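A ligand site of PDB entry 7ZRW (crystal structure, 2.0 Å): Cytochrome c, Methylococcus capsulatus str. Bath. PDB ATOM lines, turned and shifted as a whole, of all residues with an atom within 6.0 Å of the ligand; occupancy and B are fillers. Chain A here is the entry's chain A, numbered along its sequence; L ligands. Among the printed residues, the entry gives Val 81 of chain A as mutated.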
ATOM      1  N   LYS A  38     -16.779   9.957 -25.679  1.00  0.00           N
ATOM      2  CA  LYS A  38     -16.712  11.230 -26.429  1.00  0.00           C
ATOM      3  C   LYS A  38     -16.843  12.388 -25.441  1.00  0.00           C
ATOM      4  O   LYS A  38     -17.205  12.162 -24.263  1.00  0.00           O
ATOM      5  CB  LYS A  38     -17.809  11.273 -27.491  1.00  0.00           C
ATOM      6  CG  LYS A  38     -19.221  11.435 -26.972  1.00  0.00           C
ATOM      7  CD  LYS A  38     -20.253  11.771 -28.001  1.00  0.00           C
ATOM      8  CE  LYS A  38     -19.994  13.098 -28.682  1.00  0.00           C
ATOM      9  NZ  LYS A  38     -21.155  13.473 -29.515  1.00  0.00           N
ATOM     10  N   SER A  39     -16.570  13.587 -25.927  1.00  0.00           N
ATOM     11  CA  SER A  39     -16.797  14.851 -25.177  1.00  0.00           C
ATOM     12  C   SER A  39     -17.439  15.864 -26.119  1.00  0.00           C
ATOM     13  O   SER A  39     -17.370  15.690 -27.349  1.00  0.00           O
ATOM     14  CB  SER A  39     -15.534  15.364 -24.641  1.00  0.00           C
ATOM     15  OG  SER A  39     -14.935  14.408 -23.760  1.00  0.00           O
ATOM     16  N   MET A  40     -17.957  16.921 -25.524  1.00  0.00           N
ATOM     17  CA  MET A  40     -18.548  18.095 -26.225  1.00  0.00           C
ATOM     18  C   MET A  40     -18.545  19.286 -25.248  1.00  0.00           C
ATOM     19  O   MET A  40     -18.524  19.044 -24.005  1.00  0.00           O
ATOM     20  CB  MET A  40     -19.965  17.748 -26.679  1.00  0.00           C
ATOM     21  CG  MET A  40     -20.604  18.842 -27.549  1.00  0.00           C
ATOM     22  SD  MET A  40     -22.315  18.480 -27.930  1.00  0.00           S
ATOM     23  CE  MET A  40     -22.108  17.104 -29.065  1.00  0.00           C
ATOM     24  N   LEU A  48     -29.318  24.465 -25.333  1.00  0.00           N
ATOM     25  CA  LEU A  48     -29.268  23.561 -24.156  1.00  0.00           C
ATOM     26  C   LEU A  48     -28.391  24.148 -23.034  1.00  0.00           C
ATOM     27  O   LEU A  48     -28.129  23.405 -22.039  1.00  0.00           O
ATOM     28  CB  LEU A  48     -28.753  22.193 -24.611  1.00  0.00           C
ATOM     29  CG  LEU A  48     -29.618  21.478 -25.662  1.00  0.00           C
ATOM     30  CD1 LEU A  48     -29.173  20.027 -25.884  1.00  0.00           C
ATOM     31  CD2 LEU A  48     -31.101  21.529 -25.296  1.00  0.00           C
ATOM     32  N   PHE A  52     -27.482  22.150 -19.498  1.00  0.00           N
ATOM     33  CA  PHE A  52     -26.448  21.231 -20.061  1.00  0.00           C
ATOM     34  C   PHE A  52     -25.160  22.012 -20.354  1.00  0.00           C
ATOM     35  O   PHE A  52     -24.205  21.393 -20.877  1.00  0.00           O
ATOM     36  CB  PHE A  52     -26.974  20.499 -21.304  1.00  0.00           C
ATOM     37  CG  PHE A  52     -26.433  19.102 -21.605  1.00  0.00           C
ATOM     38  CD1 PHE A  52     -26.751  18.475 -22.808  1.00  0.00           C
ATOM     39  CD2 PHE A  52     -25.641  18.397 -20.715  1.00  0.00           C
ATOM     40  CE1 PHE A  52     -26.319  17.195 -23.098  1.00  0.00           C
ATOM     41  CE2 PHE A  52     -25.203  17.110 -21.009  1.00  0.00           C
ATOM     42  CZ  PHE A  52     -25.516  16.529 -22.202  1.00  0.00           C
ATOM     43  N   HIS A  56     -18.759  18.382 -21.173  1.00  0.00           N
ATOM     44  CA  HIS A  56     -19.255  17.048 -20.774  1.00  0.00           C
ATOM     45  C   HIS A  56     -18.449  15.919 -21.437  1.00  0.00           C
ATOM     46  O   HIS A  56     -17.956  16.089 -22.568  1.00  0.00           O
ATOM     47  CB  HIS A  56     -20.760  16.918 -20.954  1.00  0.00           C
ATOM     48  CG  HIS A  56     -21.258  16.742 -22.337  1.00  0.00           C
ATOM     49  ND1 HIS A  56     -21.972  17.725 -22.960  1.00  0.00           N
ATOM     50  CD2 HIS A  56     -21.226  15.682 -23.175  1.00  0.00           C
ATOM     51  CE1 HIS A  56     -22.363  17.280 -24.150  1.00  0.00           C
ATOM     52  NE2 HIS A  56     -21.934  16.033 -24.277  1.00  0.00           N
ATOM     53  N   VAL A  58     -18.705  11.650 -21.955  1.00  0.00           N
ATOM     54  CA  VAL A  58     -19.561  10.452 -21.890  1.00  0.00           C
ATOM     55  C   VAL A  58     -18.684   9.238 -21.549  1.00  0.00           C
ATOM     56  O   VAL A  58     -17.612   9.070 -22.152  1.00  0.00           O
ATOM     57  CB  VAL A  58     -20.352  10.269 -23.189  1.00  0.00           C
ATOM     58  CG1 VAL A  58     -21.260   9.050 -23.097  1.00  0.00           C
ATOM     59  CG2 VAL A  58     -21.151  11.526 -23.547  1.00  0.00           C
ATOM     60  N   LEU A  79     -24.563   4.216 -19.136  1.00  0.00           N
ATOM     61  CA  LEU A  79     -23.945   5.419 -19.767  1.00  0.00           C
ATOM     62  C   LEU A  79     -23.968   6.537 -18.742  1.00  0.00           C
ATOM     63  O   LEU A  79     -25.012   6.676 -18.002  1.00  0.00           O
ATOM     64  CB  LEU A  79     -24.753   5.761 -21.012  1.00  0.00           C
ATOM     65  CG  LEU A  79     -24.617   4.713 -22.137  1.00  0.00           C
ATOM     66  CD1 LEU A  79     -25.753   4.864 -23.138  1.00  0.00           C
ATOM     67  CD2 LEU A  79     -23.290   4.835 -22.817  1.00  0.00           C
ATOM     68  N   VAL A  80     -22.857   7.242 -18.616  1.00  0.00           N
ATOM     69  CA  VAL A  80     -22.781   8.417 -17.718  1.00  0.00           C
ATOM     70  C   VAL A  80     -22.366   9.620 -18.566  1.00  0.00           C
ATOM     71  O   VAL A  80     -21.395   9.492 -19.339  1.00  0.00           O
ATOM     72  CB  VAL A  80     -21.802   8.186 -16.571  1.00  0.00           C
ATOM     73  CG1 VAL A  80     -21.683   9.433 -15.693  1.00  0.00           C
ATOM     74  CG2 VAL A  80     -22.179   6.932 -15.800  1.00  0.00           C
ATOM     75  N   VAL A  81     -23.061  10.739 -18.387  1.00  0.00           N
ATOM     76  CA  VAL A  81     -22.577  12.033 -18.933  1.00  0.00           C
ATOM     77  C   VAL A  81     -22.137  12.886 -17.745  1.00  0.00           C
ATOM     78  O   VAL A  81     -22.960  13.131 -16.851  1.00  0.00           O
ATOM     79  CB  VAL A  81     -23.600  12.701 -19.860  1.00  0.00           C
ATOM     80  CG1 VAL A  81     -24.941  12.983 -19.176  1.00  0.00           C
ATOM     81  CG2 VAL A  81     -23.019  13.976 -20.491  1.00  0.00           C
ATOM     82  N   ILE A 101     -23.858  14.667 -12.885  1.00  0.00           N
ATOM     83  CA  ILE A 101     -23.757  13.576 -13.878  1.00  0.00           C
ATOM     84  C   ILE A 101     -25.179  13.180 -14.241  1.00  0.00           C
ATOM     85  O   ILE A 101     -26.106  13.325 -13.401  1.00  0.00           O
ATOM     86  CB  ILE A 101     -22.933  12.385 -13.366  1.00  0.00           C
ATOM     87  CG1 ILE A 101     -23.639  11.610 -12.257  1.00  0.00           C
ATOM     88  CG2 ILE A 101     -21.559  12.843 -12.934  1.00  0.00           C
ATOM     89  CD1 ILE A 101     -22.842  10.436 -11.740  1.00  0.00           C
ATOM     90  N   GLY A 102     -25.363  12.835 -15.503  1.00  0.00           N
ATOM     91  CA  GLY A 102     -26.569  12.154 -15.956  1.00  0.00           C
ATOM     92  C   GLY A 102     -26.248  10.684 -16.124  1.00  0.00           C
ATOM     93  O   GLY A 102     -25.105  10.357 -16.520  1.00  0.00           O
ATOM     94  N   VAL A 103     -27.218   9.825 -15.870  1.00  0.00           N
ATOM     95  CA  VAL A 103     -26.991   8.356 -15.851  1.00  0.00           C
ATOM     96  C   VAL A 103     -28.152   7.697 -16.580  1.00  0.00           C
ATOM     97  O   VAL A 103     -29.340   8.047 -16.290  1.00  0.00           O
ATOM     98  CB  VAL A 103     -26.805   7.813 -14.419  1.00  0.00           C
ATOM     99  CG1 VAL A 103     -26.448   6.332 -14.420  1.00  0.00           C
ATOM    100  CG2 VAL A 103     -25.771   8.638 -13.661  1.00  0.00           C
ATOM    101  N   MET A 104     -27.815   6.787 -17.487  1.00  0.00           N
ATOM    102  CA  MET A 104     -28.815   5.887 -18.126  1.00  0.00           C
ATOM    103  C   MET A 104     -28.417   4.439 -17.779  1.00  0.00           C
ATOM    104  O   MET A 104     -27.257   4.061 -18.020  1.00  0.00           O
ATOM    105  CB  MET A 104     -28.844   6.083 -19.644  1.00  0.00           C
ATOM    106  CG  MET A 104     -29.518   7.363 -20.086  1.00  0.00           C
ATOM    107  SD  MET A 104     -29.097   7.783 -21.832  1.00  0.00           S
ATOM    108  CE  MET A 104     -30.127   6.605 -22.711  1.00  0.00           C
ATOM    109  N   TYR A 119     -33.436   6.750 -16.205  1.00  0.00           N
ATOM    110  CA  TYR A 119     -32.762   8.063 -16.273  1.00  0.00           C
ATOM    111  C   TYR A 119     -32.640   8.652 -14.858  1.00  0.00           C
ATOM    112  O   TYR A 119     -33.664   8.780 -14.189  1.00  0.00           O
ATOM    113  CB  TYR A 119     -33.542   8.983 -17.211  1.00  0.00           C
ATOM    114  CG  TYR A 119     -33.531   8.578 -18.655  1.00  0.00           C
ATOM    115  CD1 TYR A 119     -34.458   7.673 -19.150  1.00  0.00           C
ATOM    116  CD2 TYR A 119     -32.607   9.117 -19.544  1.00  0.00           C
ATOM    117  CE1 TYR A 119     -34.453   7.279 -20.477  1.00  0.00           C
ATOM    118  CE2 TYR A 119     -32.605   8.749 -20.892  1.00  0.00           C
ATOM    119  CZ  TYR A 119     -33.520   7.815 -21.347  1.00  0.00           C
ATOM    120  OH  TYR A 119     -33.525   7.429 -22.653  1.00  0.00           O
ATOM    121  N   GLU A 120     -31.431   9.053 -14.448  1.00  0.00           N
ATOM    122  CA  GLU A 120     -31.194   9.746 -13.160  1.00  0.00           C
ATOM    123  C   GLU A 120     -30.100  10.784 -13.332  1.00  0.00           C
ATOM    124  O   GLU A 120     -29.207  10.617 -14.188  1.00  0.00           O
ATOM    125  CB  GLU A 120     -30.846   8.718 -12.074  1.00  0.00           C
ATOM    126  CG  GLU A 120     -30.588   9.336 -10.711  1.00  0.00           C
ATOM    127  CD  GLU A 120     -31.842   9.920 -10.091  1.00  0.00           C
ATOM    128  OE1 GLU A 120     -32.171  11.063 -10.437  1.00  0.00           O
ATOM    129  OE2 GLU A 120     -32.495   9.206  -9.307  1.00  0.00           O
ATOM    130  N   GLY A 121     -30.198  11.848 -12.530  1.00  0.00           N
ATOM    131  CA  GLY A 121     -29.142  12.859 -12.360  1.00  0.00           C
ATOM    132  C   GLY A 121     -28.660  12.898 -10.935  1.00  0.00           C
ATOM    133  O   GLY A 121     -29.473  12.632 -10.008  1.00  0.00           O
ATOM    134  N   VAL A 132     -33.926  13.577 -10.466  1.00  0.00           N
ATOM    135  CA  VAL A 132     -35.082  13.301 -11.346  1.00  0.00           C
ATOM    136  C   VAL A 132     -36.319  13.096 -10.471  1.00  0.00           C
ATOM    137  O   VAL A 132     -36.240  12.275  -9.518  1.00  0.00           O
ATOM    138  CB  VAL A 132     -34.809  12.106 -12.275  1.00  0.00           C
ATOM    139  CG1 VAL A 132     -36.073  11.542 -12.878  1.00  0.00           C
ATOM    140  CG2 VAL A 132     -33.814  12.492 -13.369  1.00  0.00           C
ATOM    141  N   GLY A 136     -38.230  10.042 -14.975  1.00  0.00           N
ATOM    142  CA  GLY A 136     -37.362  10.158 -16.164  1.00  0.00           C
ATOM    143  C   GLY A 136     -38.145  10.467 -17.437  1.00  0.00           C
ATOM    144  O   GLY A 136     -37.543  10.435 -18.496  1.00  0.00           O
ATOM    145  N   GLY A 138     -39.256  13.343 -18.586  1.00  0.00           N
ATOM    146  CA  GLY A 138     -38.600  14.503 -19.213  1.00  0.00           C
ATOM    147  C   GLY A 138     -37.343  14.102 -19.963  1.00  0.00           C
ATOM    148  O   GLY A 138     -37.119  14.548 -21.119  1.00  0.00           O
ATOM    149  N   CYS A 139     -36.484  13.300 -19.348  1.00  0.00           N
ATOM    150  CA  CYS A 139     -35.222  12.868 -19.995  1.00  0.00           C
ATOM    151  C   CYS A 139     -35.605  12.102 -21.278  1.00  0.00           C
ATOM    152  O   CYS A 139     -35.087  12.411 -22.390  1.00  0.00           O
ATOM    153  CB  CYS A 139     -34.409  11.937 -19.085  1.00  0.00           C
ATOM    154  SG  CYS A 139     -34.078  12.662 -17.485  1.00  0.00           S
ATOM    155  N   PHE A 140     -36.448  11.094 -21.100  1.00  0.00           N
ATOM    156  CA  PHE A 140     -36.921  10.175 -22.165  1.00  0.00           C
ATOM    157  C   PHE A 140     -37.558  10.970 -23.315  1.00  0.00           C
ATOM    158  O   PHE A 140     -37.333  10.574 -24.469  1.00  0.00           O
ATOM    159  CB  PHE A 140     -37.901   9.171 -21.561  1.00  0.00           C
ATOM    160  CG  PHE A 140     -38.487   8.182 -22.525  1.00  0.00           C
ATOM    161  CD1 PHE A 140     -37.670   7.418 -23.325  1.00  0.00           C
ATOM    162  CD2 PHE A 140     -39.872   8.000 -22.607  1.00  0.00           C
ATOM    163  CE1 PHE A 140     -38.218   6.490 -24.203  1.00  0.00           C
ATOM    164  CE2 PHE A 140     -40.399   7.070 -23.476  1.00  0.00           C
ATOM    165  CZ  PHE A 140     -39.575   6.308 -24.268  1.00  0.00           C
ATOM    166  N   CYS A 142     -36.746  13.709 -24.643  1.00  0.00           N
ATOM    167  CA  CYS A 142     -35.740  14.238 -25.580  1.00  0.00           C
ATOM    168  C   CYS A 142     -34.999  13.061 -26.223  1.00  0.00           C
ATOM    169  O   CYS A 142     -34.833  13.066 -27.459  1.00  0.00           O
ATOM    170  CB  CYS A 142     -34.819  15.236 -24.881  1.00  0.00           C
ATOM    171  SG  CYS A 142     -33.642  15.932 -26.003  1.00  0.00           S
ATOM    172  N   HIS A 143     -34.626  12.057 -25.424  1.00  0.00           N
ATOM    173  CA  HIS A 143     -33.883  10.864 -25.894  1.00  0.00           C
ATOM    174  C   HIS A 143     -34.732  10.054 -26.918  1.00  0.00           C
ATOM    175  O   HIS A 143     -34.123   9.284 -27.716  1.00  0.00           O
ATOM    176  CB  HIS A 143     -33.357  10.046 -24.689  1.00  0.00           C
ATOM    177  CG  HIS A 143     -32.089  10.621 -24.121  1.00  0.00           C
ATOM    178  ND1 HIS A 143     -30.860  10.032 -24.292  1.00  0.00           N
ATOM    179  CD2 HIS A 143     -31.870  11.762 -23.404  1.00  0.00           C
ATOM    180  CE1 HIS A 143     -29.928  10.794 -23.715  1.00  0.00           C
ATOM    181  NE2 HIS A 143     -30.529  11.874 -23.161  1.00  0.00           N
ATOM    182  N   TYR A 151     -32.050   5.023 -28.178  1.00  0.00           N
ATOM    183  CA  TYR A 151     -32.250   6.198 -27.299  1.00  0.00           C
ATOM    184  C   TYR A 151     -30.930   6.816 -26.836  1.00  0.00           C
ATOM    185  O   TYR A 151     -30.954   7.651 -25.880  1.00  0.00           O
ATOM    186  CB  TYR A 151     -33.105   5.832 -26.090  1.00  0.00           C
ATOM    187  CG  TYR A 151     -34.442   5.285 -26.473  1.00  0.00           C
ATOM    188  CD1 TYR A 151     -35.417   6.117 -27.001  1.00  0.00           C
ATOM    189  CD2 TYR A 151     -34.721   3.930 -26.330  1.00  0.00           C
ATOM    190  CE1 TYR A 151     -36.662   5.621 -27.345  1.00  0.00           C
ATOM    191  CE2 TYR A 151     -35.960   3.428 -26.679  1.00  0.00           C
ATOM    192  CZ  TYR A 151     -36.931   4.272 -27.172  1.00  0.00           C
ATOM    193  OH  TYR A 151     -38.160   3.780 -27.520  1.00  0.00           O
ATOM    194  N   VAL A 152     -29.845   6.454 -27.505  1.00  0.00           N
ATOM    195  CA  VAL A 152     -28.473   6.943 -27.194  1.00  0.00           C
ATOM    196  C   VAL A 152     -28.053   7.914 -28.302  1.00  0.00           C
ATOM    197  O   VAL A 152     -28.155   7.530 -29.474  1.00  0.00           O
ATOM    198  CB  VAL A 152     -27.517   5.767 -27.052  1.00  0.00           C
ATOM    199  CG1 VAL A 152     -26.102   6.249 -26.809  1.00  0.00           C
ATOM    200  CG2 VAL A 152     -27.997   4.810 -25.963  1.00  0.00           C
ATOM    201  N   PHE A 153     -27.659   9.145 -27.935  1.00  0.00           N
ATOM    202  CA  PHE A 153     -27.138  10.162 -28.884  1.00  0.00           C
ATOM    203  C   PHE A 153     -25.691   9.857 -29.251  1.00  0.00           C
ATOM    204  O   PHE A 153     -25.337   9.973 -30.416  1.00  0.00           O
ATOM    205  CB  PHE A 153     -27.193  11.562 -28.270  1.00  0.00           C
ATOM    206  CG  PHE A 153     -28.565  12.150 -28.174  1.00  0.00           C
ATOM    207  CD1 PHE A 153     -29.292  12.048 -26.982  1.00  0.00           C
ATOM    208  CD2 PHE A 153     -29.151  12.804 -29.244  1.00  0.00           C
ATOM    209  CE1 PHE A 153     -30.568  12.613 -26.872  1.00  0.00           C
ATOM    210  CE2 PHE A 153     -30.417  13.371 -29.144  1.00  0.00           C
ATOM    211  CZ  PHE A 153     -31.117  13.290 -27.943  1.00  0.00           C
ATOM    212  N   SER A 154     -24.862   9.518 -28.267  1.00  0.00           N
ATOM    213  CA  SER A 154     -23.402   9.399 -28.420  1.00  0.00           C
ATOM    214  C   SER A 154     -23.089   8.277 -29.423  1.00  0.00           C
ATOM    215  O   SER A 154     -23.756   7.232 -29.373  1.00  0.00           O
ATOM    216  CB  SER A 154     -22.730   9.179 -27.069  1.00  0.00           C
ATOM    217  OG  SER A 154     -22.966  10.288 -26.192  1.00  0.00           O
ATOM    218  N   ARG A 155     -22.105   8.496 -30.301  1.00  0.00           N
ATOM    219  CA  ARG A 155     -21.551   7.468 -31.222  1.00  0.00           C
ATOM    220  C   ARG A 155     -20.116   7.181 -30.819  1.00  0.00           C
ATOM    221  O   ARG A 155     -19.332   8.143 -30.516  1.00  0.00           O
ATOM    222  CB  ARG A 155     -21.537   7.924 -32.691  1.00  0.00           C
ATOM    223  CG  ARG A 155     -22.906   8.295 -33.240  1.00  0.00           C
ATOM    224  CD  ARG A 155     -23.894   7.148 -33.263  1.00  0.00           C
ATOM    225  NE  ARG A 155     -25.186   7.715 -33.634  1.00  0.00           N
ATOM    226  CZ  ARG A 155     -26.287   7.735 -32.873  1.00  0.00           C
ATOM    227  NH1 ARG A 155     -26.319   7.158 -31.676  1.00  0.00           N
ATOM    228  NH2 ARG A 155     -27.371   8.328 -33.323  1.00  0.00           N
HETATM  229 FE1  LIG L   1     -29.439  13.381 -22.241  1.00  0.00          FE
HETATM  230  C1  LIG L   1     -26.527  12.506 -23.688  1.00  0.00           C
HETATM  231  C2  LIG L   1     -28.756  11.433 -19.537  1.00  0.00           C
HETATM  232  C3  LIG L   1     -32.017  14.724 -20.590  1.00  0.00           C
HETATM  233  C4  LIG L   1     -30.042  15.428 -24.853  1.00  0.00           C
HETATM  234  N1  LIG L   1     -27.873  12.246 -21.675  1.00  0.00           N
HETATM  235  C5  LIG L   1     -26.817  11.889 -22.445  1.00  0.00           C
HETATM  236  C6  LIG L   1     -26.137  10.788 -21.908  1.00  0.00           C
HETATM  237  C7  LIG L   1     -26.791  10.490 -20.712  1.00  0.00           C
HETATM  238  C8  LIG L   1     -27.838  11.376 -20.621  1.00  0.00           C
HETATM  239  C9  LIG L   1     -26.356   9.455 -19.721  1.00  0.00           C
HETATM  240  C10 LIG L   1     -24.999  10.040 -22.551  1.00  0.00           C
HETATM  241  C11 LIG L   1     -25.528   8.908 -23.471  1.00  0.00           C
HETATM  242  C12 LIG L   1     -26.093   9.399 -24.808  1.00  0.00           C
HETATM  243  O1  LIG L   1     -25.332   9.974 -25.596  1.00  0.00           O
HETATM  244  O2  LIG L   1     -27.303   9.228 -25.046  1.00  0.00           O
HETATM  245  N2  LIG L   1     -30.232  13.164 -20.328  1.00  0.00           N
HETATM  246  C13 LIG L   1     -29.871  12.290 -19.387  1.00  0.00           C
HETATM  247  C14 LIG L   1     -30.695  12.373 -18.245  1.00  0.00           C
HETATM  248  C15 LIG L   1     -31.639  13.386 -18.503  1.00  0.00           C
HETATM  249  C16 LIG L   1     -31.276  13.808 -19.813  1.00  0.00           C
HETATM  250  C17 LIG L   1     -30.468  11.571 -16.999  1.00  0.00           C
HETATM  251  C18 LIG L   1     -32.803  13.878 -17.628  1.00  0.00           C
HETATM  252  C19 LIG L   1     -32.305  14.268 -16.214  1.00  0.00           C
HETATM  253  N3  LIG L   1     -30.691  14.905 -22.631  1.00  0.00           N
HETATM  254  C20 LIG L   1     -31.777  15.246 -21.883  1.00  0.00           C
HETATM  255  C21 LIG L   1     -32.656  16.127 -22.532  1.00  0.00           C
HETATM  256  C22 LIG L   1     -32.118  16.325 -23.826  1.00  0.00           C
HETATM  257  C23 LIG L   1     -30.933  15.554 -23.786  1.00  0.00           C
HETATM  258  C24 LIG L   1     -33.894  16.672 -21.900  1.00  0.00           C
HETATM  259  C25 LIG L   1     -32.640  17.069 -25.056  1.00  0.00           C
HETATM  260  C26 LIG L   1     -33.449  18.347 -24.746  1.00  0.00           C
HETATM  261  N4  LIG L   1     -28.374  14.006 -23.857  1.00  0.00           N
HETATM  262  C27 LIG L   1     -28.780  14.830 -24.839  1.00  0.00           C
HETATM  263  C28 LIG L   1     -27.879  14.963 -25.881  1.00  0.00           C
HETATM  264  C29 LIG L   1     -26.834  14.137 -25.564  1.00  0.00           C
HETATM  265  C30 LIG L   1     -27.213  13.544 -24.328  1.00  0.00           C
HETATM  266  C31 LIG L   1     -28.006  15.832 -27.101  1.00  0.00           C
HETATM  267  C32 LIG L   1     -25.572  13.931 -26.392  1.00  0.00           C
HETATM  268  C33 LIG L   1     -24.368  14.737 -25.919  1.00  0.00           C
HETATM  269  C34 LIG L   1     -23.123  14.455 -26.751  1.00  0.00           C
HETATM  270  O3  LIG L   1     -21.956  14.792 -26.381  1.00  0.00           O
HETATM  271  O4  LIG L   1     -23.273  13.856 -27.882  1.00  0.00           O
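The backbone carbonyl oxygen of Phe 153 lies within hydrogen-bond range of the guanidinium group of Arg 155, at 3.2 Å.
The backbone NH (N) of His 56 sits at hydrogen-bond distance from the backbone carbonyl oxygen (O) of Met 40 (2.9 Å).
The side-chain carboxylate (OE1) of Glu 120 sits at hydrogen-bond distance from the backbone NH (N) of Val 132 (3.1 Å).
The backbone NH (N) of Val 103 lies within hydrogen-bond range of the backbone carbonyl oxygen (O) of Glu 120 (2.7 Å).
N of Val 58 is in hydrogen-bond range of O of Lys 38, 2.8 Å away.
The backbone carbonyl oxygen (O) of Val 152 is in hydrogen-bond range of the guanidinium group (NH1) of Arg 155, 2.9 Å away.
O of Val 81 lies within hydrogen-bond range of N of Gly 102 (2.8 Å).
ND1 of His 143 sits at hydrogen-bond distance from O of Tyr 151.
Met 40 touches the ligand.
CD2 of Leu 48 touches C26 of the ligand, 3.99 Å away.
Phe 52 touches the ligand.
Val 58 touches the ligand.
Leu 79 touches the ligand (O to C9, 3.5 Å).
Val 81 touches the ligand (CG1 to C7, 3.5 Å).
Gly 102 touches the ligand.
O of Val 103 touches C17 of the ligand (3.8 Å).
SD of Met 104 touches C7 of the ligand (3.7 Å).
Tyr 119 touches the ligand (CD2 to C14, 3.99 Å).
Glu 120 touches the ligand.
Val 132 touches the ligand (CG2 to C19, 3.7 Å).
Gly 138 touches the ligand (O to C24, 3.9 Å).
Val 152 touches the ligand.
Hydrophobic or aromatic side chains that line the ligand: Met 40, Leu 48, Phe 52, His 56, Val 58, Val 81, Met 104, Tyr 119, Val 132, His 143, Val 152 and Phe 153.
The nearest printed residue that does not touch the ligand is Tyr 151 (4.1 Å).
A ring nitrogen (NE2) of His 56 lies within hydrogen-bond range of an oxygen (O3) of the ligand.
O1 of the ligand sits at hydrogen-bond distance from OG of Ser 154 (2.5 Å).
The side-chain amino group (NZ) of Lys 38 lies within salt-bridge range of an oxygen (O4) of the ligand, at 2.7 Å.
The side-chain sulfur of Cys 142 is covalently linked to a carbon (C25) of the ligand (1.8 Å).
O1 of the ligand sits at hydrogen-bond distance from N of Ser 154 (2.8 Å).
The backbone NH (N) of Phe 153 lies within hydrogen-bond range of an oxygen (O2) of the ligand, at 2.9 Å.
An iron atom (FE1) of the ligand is bound by a ring nitrogen (NE2) of His 143, 2.1 Å away.
The side-chain sulfur (SG) of Cys 139 is bonded to a carbon (C18) of the ligand (1.8 Å).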
